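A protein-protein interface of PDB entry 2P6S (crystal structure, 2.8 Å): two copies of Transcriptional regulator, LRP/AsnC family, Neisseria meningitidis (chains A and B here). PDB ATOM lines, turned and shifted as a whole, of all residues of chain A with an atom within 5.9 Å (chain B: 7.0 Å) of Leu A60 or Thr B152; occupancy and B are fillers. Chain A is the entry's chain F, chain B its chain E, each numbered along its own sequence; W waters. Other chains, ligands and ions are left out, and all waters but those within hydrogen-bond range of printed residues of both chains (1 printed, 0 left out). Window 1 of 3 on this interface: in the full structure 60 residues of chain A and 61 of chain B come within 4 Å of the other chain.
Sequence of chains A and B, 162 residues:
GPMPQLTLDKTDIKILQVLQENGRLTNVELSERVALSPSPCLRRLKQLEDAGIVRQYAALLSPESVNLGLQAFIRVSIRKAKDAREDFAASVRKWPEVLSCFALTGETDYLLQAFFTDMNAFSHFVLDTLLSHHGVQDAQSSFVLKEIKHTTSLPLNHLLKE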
ATOM      1  N   ARG A  55      -1.304 -12.241  -1.039  1.00  0.00           N
ATOM      2  CA  ARG A  55      -1.610 -10.815  -1.171  1.00  0.00           C
ATOM      3  C   ARG A  55      -1.302 -10.046   0.103  1.00  0.00           C
ATOM      4  O   ARG A  55      -0.655  -9.000   0.073  1.00  0.00           O
ATOM      5  CB  ARG A  55      -3.090 -10.620  -1.465  1.00  0.00           C
ATOM      6  CG  ARG A  55      -3.581 -11.178  -2.790  1.00  0.00           C
ATOM      7  CD  ARG A  55      -5.102 -11.267  -2.782  1.00  0.00           C
ATOM      8  NE  ARG A  55      -5.704 -10.171  -2.020  1.00  0.00           N
ATOM      9  CZ  ARG A  55      -6.862 -10.241  -1.365  1.00  0.00           C
ATOM     10  NH1 ARG A  55      -7.598 -11.353  -1.363  1.00  0.00           N
ATOM     11  NH2 ARG A  55      -7.289  -9.176  -0.698  1.00  0.00           N
ATOM     12  N   GLN A  56      -1.812 -10.559   1.218  1.00  0.00           N
ATOM     13  CA  GLN A  56      -1.592  -9.955   2.522  1.00  0.00           C
ATOM     14  C   GLN A  56      -1.894 -10.948   3.626  1.00  0.00           C
ATOM     15  O   GLN A  56      -2.558 -11.959   3.400  1.00  0.00           O
ATOM     16  CB  GLN A  56      -2.473  -8.717   2.706  1.00  0.00           C
ATOM     17  CG  GLN A  56      -3.991  -8.994   2.687  1.00  0.00           C
ATOM     18  CD  GLN A  56      -4.819  -7.918   3.386  1.00  0.00           C
ATOM     19  OE1 GLN A  56      -6.006  -7.760   3.102  1.00  0.00           O
ATOM     20  NE2 GLN A  56      -4.198  -7.183   4.310  1.00  0.00           N
ATOM     21  N   ALA A  58      -3.807 -11.056   7.269  1.00  0.00           N
ATOM     22  CA  ALA A  58      -4.838 -10.288   7.967  1.00  0.00           C
ATOM     23  C   ALA A  58      -5.388 -11.027   9.188  1.00  0.00           C
ATOM     24  O   ALA A  58      -5.595 -12.245   9.158  1.00  0.00           O
ATOM     25  CB  ALA A  58      -5.976  -9.953   7.009  1.00  0.00           C
ATOM     26  N   ALA A  59      -5.617 -10.273  10.261  1.00  0.00           N
ATOM     27  CA  ALA A  59      -6.340 -10.778  11.416  1.00  0.00           C
ATOM     28  C   ALA A  59      -7.820 -10.641  11.110  1.00  0.00           C
ATOM     29  O   ALA A  59      -8.282  -9.553  10.754  1.00  0.00           O
ATOM     30  CB  ALA A  59      -5.983  -9.987  12.667  1.00  0.00           C
ATOM     31  N   LEU A  60      -8.547 -11.752  11.213  1.00  0.00           N
ATOM     32  CA  LEU A  60      -9.992 -11.767  10.998  1.00  0.00           C
ATOM     33  C   LEU A  60     -10.701 -11.641  12.341  1.00  0.00           C
ATOM     34  O   LEU A  60     -10.426 -12.409  13.263  1.00  0.00           O
ATOM     35  CB  LEU A  60     -10.425 -13.057  10.297  1.00  0.00           C
ATOM     36  CG  LEU A  60      -9.610 -13.448   9.067  1.00  0.00           C
ATOM     37  CD1 LEU A  60     -10.252 -14.642   8.374  1.00  0.00           C
ATOM     38  CD2 LEU A  60      -9.454 -12.271   8.097  1.00  0.00           C
ATOM     39  N   LEU A  61     -11.615 -10.676  12.433  1.00  0.00           N
ATOM     40  CA  LEU A  61     -12.326 -10.372  13.674  1.00  0.00           C
ATOM     41  C   LEU A  61     -13.758 -10.904  13.652  1.00  0.00           C
ATOM     42  O   LEU A  61     -14.242 -11.371  12.621  1.00  0.00           O
ATOM     43  CB  LEU A  61     -12.341  -8.863  13.909  1.00  0.00           C
ATOM     44  CG  LEU A  61     -10.969  -8.196  13.973  1.00  0.00           C
ATOM     45  CD1 LEU A  61     -11.136  -6.717  14.257  1.00  0.00           C
ATOM     46  CD2 LEU A  61     -10.093  -8.840  15.032  1.00  0.00           C
ATOM     47  N   SER A  62     -14.423 -10.837  14.800  1.00  0.00           N
ATOM     48  CA  SER A  62     -15.814 -11.253  14.913  1.00  0.00           C
ATOM     49  C   SER A  62     -16.717 -10.024  14.901  1.00  0.00           C
ATOM     50  O   SER A  62     -16.652  -9.200  15.813  1.00  0.00           O
ATOM     51  CB  SER A  62     -16.039 -12.063  16.199  1.00  0.00           C
ATOM     52  OG  SER A  62     -17.412 -12.079  16.575  1.00  0.00           O
ATOM     53  N   LEU A  99     -17.119  -3.586   2.919  1.00  0.00           N
ATOM     54  CA  LEU A  99     -15.938  -4.456   2.882  1.00  0.00           C
ATOM     55  C   LEU A  99     -15.551  -4.873   1.463  1.00  0.00           C
ATOM     56  O   LEU A  99     -14.381  -4.763   1.082  1.00  0.00           O
ATOM     57  CB  LEU A  99     -16.133  -5.704   3.763  1.00  0.00           C
ATOM     58  CG  LEU A  99     -15.790  -5.506   5.247  1.00  0.00           C
ATOM     59  CD1 LEU A  99     -16.754  -4.505   5.885  1.00  0.00           C
ATOM     60  CD2 LEU A  99     -15.776  -6.824   6.026  1.00  0.00           C
ATOM     61  N   THR A 152     -11.856 -17.540   4.445  1.00  0.00           N
ATOM     62  CA  THR A 152     -11.077 -16.756   3.493  1.00  0.00           C
ATOM     63  C   THR A 152     -10.212 -17.684   2.625  1.00  0.00           C
ATOM     64  O   THR A 152      -9.598 -17.246   1.642  1.00  0.00           O
ATOM     65  CB  THR A 152     -10.174 -15.737   4.218  1.00  0.00           C
ATOM     66  OG1 THR A 152      -8.901 -16.328   4.516  1.00  0.00           O
ATOM     67  CG2 THR A 152     -10.838 -15.245   5.505  1.00  0.00           C
ATOM     68  N   LEU B  19      -3.623  -4.760  12.992  1.00  0.00           N
ATOM     69  CA  LEU B  19      -3.509  -6.194  12.740  1.00  0.00           C
ATOM     70  C   LEU B  19      -4.351  -6.661  11.555  1.00  0.00           C
ATOM     71  O   LEU B  19      -3.908  -7.509  10.781  1.00  0.00           O
ATOM     72  CB  LEU B  19      -3.899  -7.007  13.984  1.00  0.00           C
ATOM     73  CG  LEU B  19      -2.908  -7.142  15.143  1.00  0.00           C
ATOM     74  CD1 LEU B  19      -3.267  -8.388  15.940  1.00  0.00           C
ATOM     75  CD2 LEU B  19      -1.472  -7.219  14.669  1.00  0.00           C
ATOM     76  N   GLN B  20      -5.559  -6.119  11.425  1.00  0.00           N
ATOM     77  CA  GLN B  20      -6.457  -6.488  10.329  1.00  0.00           C
ATOM     78  C   GLN B  20      -5.781  -6.310   8.966  1.00  0.00           C
ATOM     79  O   GLN B  20      -6.009  -7.108   8.056  1.00  0.00           O
ATOM     80  CB  GLN B  20      -7.753  -5.663  10.379  1.00  0.00           C
ATOM     81  CG  GLN B  20      -8.698  -6.036  11.510  1.00  0.00           C
ATOM     82  CD  GLN B  20     -10.139  -5.605  11.262  1.00  0.00           C
ATOM     83  OE1 GLN B  20     -11.054  -6.429  11.277  1.00  0.00           O
ATOM     84  NE2 GLN B  20     -10.347  -4.311  11.041  1.00  0.00           N
ATOM     85  N   GLU B  21      -4.949  -5.269   8.842  1.00  0.00           N
ATOM     86  CA  GLU B  21      -4.270  -4.931   7.581  1.00  0.00           C
ATOM     87  C   GLU B  21      -2.918  -5.638   7.447  1.00  0.00           C
ATOM     88  O   GLU B  21      -2.595  -6.171   6.381  1.00  0.00           O
ATOM     89  CB  GLU B  21      -4.072  -3.410   7.460  1.00  0.00           C
ATOM     90  CG  GLU B  21      -5.336  -2.569   7.674  1.00  0.00           C
ATOM     91  CD  GLU B  21      -6.378  -2.777   6.591  1.00  0.00           C
ATOM     92  OE1 GLU B  21      -6.100  -2.425   5.429  1.00  0.00           O
ATOM     93  OE2 GLU B  21      -7.478  -3.281   6.903  1.00  0.00           O
ATOM     94  N   GLY B  52     -12.309 -13.502  22.136  1.00  0.00           N
ATOM     95  CA  GLY B  52     -13.028 -13.969  20.957  1.00  0.00           C
ATOM     96  C   GLY B  52     -13.087 -12.911  19.872  1.00  0.00           C
ATOM     97  O   GLY B  52     -13.721 -13.126  18.840  1.00  0.00           O
ATOM     98  N   ILE B  53     -12.417 -11.778  20.101  1.00  0.00           N
ATOM     99  CA  ILE B  53     -12.420 -10.646  19.162  1.00  0.00           C
ATOM    100  C   ILE B  53     -11.703 -11.068  17.879  1.00  0.00           C
ATOM    101  O   ILE B  53     -12.296 -11.057  16.804  1.00  0.00           O
ATOM    102  CB  ILE B  53     -11.742  -9.363  19.760  1.00  0.00           C
ATOM    103  CG1 ILE B  53     -12.583  -8.724  20.872  1.00  0.00           C
ATOM    104  CG2 ILE B  53     -11.514  -8.311  18.682  1.00  0.00           C
ATOM    105  CD1 ILE B  53     -13.445  -9.681  21.663  1.00  0.00           C
ATOM    106  N   VAL B  54     -10.434 -11.445  18.006  1.00  0.00           N
ATOM    107  CA  VAL B  54      -9.690 -12.028  16.898  1.00  0.00           C
ATOM    108  C   VAL B  54     -10.077 -13.490  16.790  1.00  0.00           C
ATOM    109  O   VAL B  54      -9.815 -14.271  17.706  1.00  0.00           O
ATOM    110  CB  VAL B  54      -8.174 -11.948  17.114  1.00  0.00           C
ATOM    111  CG1 VAL B  54      -7.452 -12.633  15.974  1.00  0.00           C
ATOM    112  CG2 VAL B  54      -7.720 -10.498  17.255  1.00  0.00           C
ATOM    113  N   ARG B  55     -10.706 -13.859  15.678  1.00  0.00           N
ATOM    114  CA  ARG B  55     -11.166 -15.235  15.490  1.00  0.00           C
ATOM    115  C   ARG B  55     -10.119 -16.102  14.803  1.00  0.00           C
ATOM    116  O   ARG B  55     -10.041 -17.305  15.065  1.00  0.00           O
ATOM    117  CB  ARG B  55     -12.512 -15.294  14.755  1.00  0.00           C
ATOM    118  CG  ARG B  55     -12.575 -14.657  13.381  1.00  0.00           C
ATOM    119  CD  ARG B  55     -14.016 -14.682  12.859  1.00  0.00           C
ATOM    120  NE  ARG B  55     -14.119 -14.233  11.471  1.00  0.00           N
ATOM    121  CZ  ARG B  55     -13.773 -14.962  10.412  1.00  0.00           C
ATOM    122  NH1 ARG B  55     -13.295 -16.199  10.551  1.00  0.00           N
ATOM    123  NH2 ARG B  55     -13.906 -14.444   9.197  1.00  0.00           N
ATOM    124  N   GLN B  56      -9.321 -15.497  13.926  1.00  0.00           N
ATOM    125  CA  GLN B  56      -8.139 -16.161  13.379  1.00  0.00           C
ATOM    126  C   GLN B  56      -7.256 -15.208  12.602  1.00  0.00           C
ATOM    127  O   GLN B  56      -7.700 -14.155  12.141  1.00  0.00           O
ATOM    128  CB  GLN B  56      -8.508 -17.324  12.459  1.00  0.00           C
ATOM    129  CG  GLN B  56      -9.455 -16.956  11.340  1.00  0.00           C
ATOM    130  CD  GLN B  56      -9.574 -18.040  10.298  1.00  0.00           C
ATOM    131  OE1 GLN B  56     -10.631 -18.215   9.689  1.00  0.00           O
ATOM    132  NE2 GLN B  56      -8.489 -18.773  10.079  1.00  0.00           N
ATOM    133  N   TYR B  57      -5.999 -15.600  12.462  1.00  0.00           N
ATOM    134  CA  TYR B  57      -5.082 -14.932  11.560  1.00  0.00           C
ATOM    135  C   TYR B  57      -5.069 -15.769  10.293  1.00  0.00           C
ATOM    136  O   TYR B  57      -5.195 -16.994  10.351  1.00  0.00           O
ATOM    137  CB  TYR B  57      -3.705 -14.814  12.202  1.00  0.00           C
ATOM    138  CG  TYR B  57      -3.750 -13.993  13.471  1.00  0.00           C
ATOM    139  CD1 TYR B  57      -3.531 -12.619  13.442  1.00  0.00           C
ATOM    140  CD2 TYR B  57      -4.057 -14.582  14.696  1.00  0.00           C
ATOM    141  CE1 TYR B  57      -3.589 -11.860  14.597  1.00  0.00           C
ATOM    142  CE2 TYR B  57      -4.122 -13.829  15.856  1.00  0.00           C
ATOM    143  CZ  TYR B  57      -3.881 -12.471  15.798  1.00  0.00           C
ATOM    144  OH  TYR B  57      -3.936 -11.718  16.948  1.00  0.00           O
ATOM    145  N   ALA B  58      -4.959 -15.111   9.147  1.00  0.00           N
ATOM    146  CA  ALA B  58      -5.121 -15.798   7.878  1.00  0.00           C
ATOM    147  C   ALA B  58      -4.229 -15.209   6.802  1.00  0.00           C
ATOM    148  O   ALA B  58      -4.102 -13.989   6.693  1.00  0.00           O
ATOM    149  CB  ALA B  58      -6.576 -15.731   7.443  1.00  0.00           C
ATOM    150  N   LEU B  60      -3.997 -14.398   3.117  1.00  0.00           N
ATOM    151  CA  LEU B  60      -4.950 -14.162   2.040  1.00  0.00           C
ATOM    152  C   LEU B  60      -4.253 -14.317   0.695  1.00  0.00           C
ATOM    153  O   LEU B  60      -3.151 -13.807   0.507  1.00  0.00           O
ATOM    154  CB  LEU B  60      -5.575 -12.783   2.200  1.00  0.00           C
ATOM    155  CG  LEU B  60      -6.491 -12.741   3.423  1.00  0.00           C
ATOM    156  CD1 LEU B  60      -6.568 -11.356   4.042  1.00  0.00           C
ATOM    157  CD2 LEU B  60      -7.877 -13.250   3.045  1.00  0.00           C
ATOM    158  N   HIS B 150     -12.405  -5.191  -2.188  1.00  0.00           N
ATOM    159  CA  HIS B 150     -12.422  -6.407  -1.383  1.00  0.00           C
ATOM    160  C   HIS B 150     -11.426  -6.293  -0.228  1.00  0.00           C
ATOM    161  O   HIS B 150     -10.222  -6.470  -0.408  1.00  0.00           O
ATOM    162  CB  HIS B 150     -12.101  -7.630  -2.248  1.00  0.00           C
ATOM    163  CG  HIS B 150     -12.283  -8.936  -1.538  1.00  0.00           C
ATOM    164  ND1 HIS B 150     -13.261  -9.138  -0.585  1.00  0.00           N
ATOM    165  CD2 HIS B 150     -11.630 -10.117  -1.660  1.00  0.00           C
ATOM    166  CE1 HIS B 150     -13.190 -10.379  -0.138  1.00  0.00           C
ATOM    167  NE2 HIS B 150     -12.210 -10.994  -0.775  1.00  0.00           N
ATOM    168  N   THR B 151     -11.940  -5.958   0.951  1.00  0.00           N
ATOM    169  CA  THR B 151     -11.150  -6.003   2.179  1.00  0.00           C
ATOM    170  C   THR B 151     -11.786  -6.991   3.153  1.00  0.00           C
ATOM    171  O   THR B 151     -12.997  -7.234   3.104  1.00  0.00           O
ATOM    172  CB  THR B 151     -11.025  -4.624   2.857  1.00  0.00           C
ATOM    173  OG1 THR B 151     -10.344  -4.771   4.106  1.00  0.00           O
ATOM    174  CG2 THR B 151     -12.388  -4.006   3.119  1.00  0.00           C
ATOM    175  N   THR B 152     -10.959  -7.569   4.021  1.00  0.00           N
ATOM    176  CA  THR B 152     -11.445  -8.457   5.071  1.00  0.00           C
ATOM    177  C   THR B 152     -11.649  -7.661   6.361  1.00  0.00           C
ATOM    178  O   THR B 152     -12.141  -8.195   7.357  1.00  0.00           O
ATOM    179  CB  THR B 152     -10.461  -9.604   5.324  1.00  0.00           C
ATOM    180  OG1 THR B 152      -9.281  -9.100   5.964  1.00  0.00           O
ATOM    181  CG2 THR B 152     -10.078 -10.275   4.005  1.00  0.00           C
ATOM    182  N   SER B 153     -11.307  -6.374   6.302  1.00  0.00           N
ATOM    183  CA  SER B 153     -11.169  -5.513   7.472  1.00  0.00           C
ATOM    184  C   SER B 153     -12.494  -4.865   7.861  1.00  0.00           C
ATOM    185  O   SER B 153     -13.104  -4.163   7.054  1.00  0.00           O
ATOM    186  CB  SER B 153     -10.132  -4.430   7.158  1.00  0.00           C
ATOM    187  OG  SER B 153      -9.634  -3.820   8.327  1.00  0.00           O
ATOM    188  N   LEU B 154     -12.934  -5.106   9.095  1.00  0.00           N
ATOM    189  CA  LEU B 154     -14.168  -4.517   9.610  1.00  0.00           C
ATOM    190  C   LEU B 154     -13.895  -3.104  10.101  1.00  0.00           C
ATOM    191  O   LEU B 154     -12.788  -2.825  10.562  1.00  0.00           O
ATOM    192  CB  LEU B 154     -14.712  -5.327  10.790  1.00  0.00           C
ATOM    193  CG  LEU B 154     -15.366  -6.685  10.566  1.00  0.00           C
ATOM    194  CD1 LEU B 154     -15.898  -7.205  11.888  1.00  0.00           C
ATOM    195  CD2 LEU B 154     -16.484  -6.588   9.542  1.00  0.00           C
HETATM  196  O   HOH W   1     -10.178 -18.572   6.962  1.00  0.00           O
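The backbone NH (N) of Arg B55 lies within hydrogen-bond range of the backbone carbonyl oxygen (O) of Leu A60. The backbone carbonyl oxygen of Leu B19 is in hydrogen-bond range of the backbone NH of Ala A59, at 3.3 Å. The backbone carbonyl oxygen (O) of Leu B60 lies within hydrogen-bond range of the backbone NH (N) of Arg A55 (2.9 Å). The guanidinium group (NE) of Arg B55 sits at hydrogen-bond distance from the backbone carbonyl oxygen (O) of Leu A61. The backbone carbonyl oxygen (O) of Ile B53 sits at hydrogen-bond distance from the backbone NH (N) of Ser A62, 2.9 Å away. The backbone carbonyl oxygen (O) of Glu B21 lies within hydrogen-bond range of the side-chain amide nitrogen (NE2) of Gln A56 (2.8 Å). The backbone NH of Ala B58 lies within hydrogen-bond range of the backbone carbonyl oxygen of Ala A58. The backbone carbonyl oxygen (O) of Gln B56 lies within hydrogen-bond range of the backbone NH (N) of Leu A60 (2.7 Å). The backbone carbonyl oxygen (O) of Gln A56 lies within hydrogen-bond range of the backbone NH (N) of Leu B60, at 2.8 Å. The backbone carbonyl oxygen of Leu A99 is in hydrogen-bond range of the backbone NH of Thr B151 (2.7 Å).
The backbone NH (N) of Ser B153 sits at hydrogen-bond distance from the side-chain hydroxyl (OG1) of Thr B151, 2.9 Å away. OG of Ser B153 lies within hydrogen-bond range of NE2 of Gln B20. NE2 of Gln B20 lies within hydrogen-bond range of O of Leu B154. NH1 of Arg B55 sits at hydrogen-bond distance from OE1 of Gln B56 (3.5 Å). The side-chain carboxylate of Glu B21 lies within hydrogen-bond range of the side-chain hydroxyl of Ser B153 (2.6 Å).
Among the printed residues, merely in contact across the chains: Ala A58 with Gln B20 (3.0 Å), Ala A58 with Tyr B57 (3.6 Å), Ala A58 with Leu B60 (3.3 Å), Ala A58 with Thr B152 (3.6 Å), Ala A59 with Gln B20 (3.6 Å), Ala A59 with Gln B56 (3.7 Å), Ala A59 with Tyr B57 (3.6 Å), Leu A60 with Val B54 (3.7 Å), Leu A60 with Ala B58 (3.9 Å), Leu A60 with Thr B152 (3.8 Å), Leu A61 with Gln B20 (3.0 Å), Leu A61 with Ile B53 (3.2 Å), Leu A61 with Val B54 (3.6 Å), Ser A62 with Gly B52 (3.7 Å), Leu A99 with His B150 (3.6 Å), Leu A99 with Ser B153 (3.5 Å), Leu A99 with Leu B154 (3.6 Å), Thr A152 with Ala B58 (3.8 Å) and Thr A152 with Leu B60 (3.6 Å).
Printed residues of chain B within 4 Å of Gln A56: Glu B21 and Leu B60. Of chain B, only Val B54, Arg B55, Gln B56, Ala B58 and Thr B152 come within 4 Å of Leu A60. Of the printed residues of chain B, Leu A61 touches Gln B20, Ile B53, Val B54 and Arg B55. Printed residues of chain B within 4 Å of Thr A152: Ala B58 (3.8 Å) and Leu B60 (3.6 Å). Printed residues of chain A within 4 Å of Tyr B57: Ala A58 and Ala A59. Thr B152 touches two residues of chain A. The nearest residue of chain B that does not touch Leu A60 is Ile B53 (4.2 Å). The nearest printed residue of chain B that does not touch Leu A99 is Thr B152 (4.1 Å).
Hydrophobic or aromatic side chains of chain A that line the printed part of chain B: Ala A58, Ala A59, Leu A60, Leu A61 and Leu A99. Of the 16 printed residues of chain B, 16 touch a printed residue of chain A. Hydrophobic or aromatic side chains of chain B that line the printed part of chain A: Leu B19, Ile B53, Val B54, Tyr B57, Ala B58, Leu B60 and Leu B154. Among the printed residues, 29 pairs touch across the chains. Among the printed residues, no Asp or Glu carboxylate lies within 4 Å of a Lys or Arg side-chain nitrogen of the other chain.
Arg A55 touches Leu B60, and with the chains exchanged Leu A60 touches Arg B55. Ala B58 touches its own counterpart, Ala A58. Ala A58 touches Leu B60, and with the chains exchanged Leu A60 touches Ala B58. Ala A58 touches Thr B152, and with the chains exchanged Thr A152 touches Ala B58. Of the 29 pairs that touch across the chains among the printed residues, 11 have their exchanged pair printed and touching as well.
Water W1 bridges OE1 of Gln B56 (2.8 Å) and N of Thr A152 (3.2 Å).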
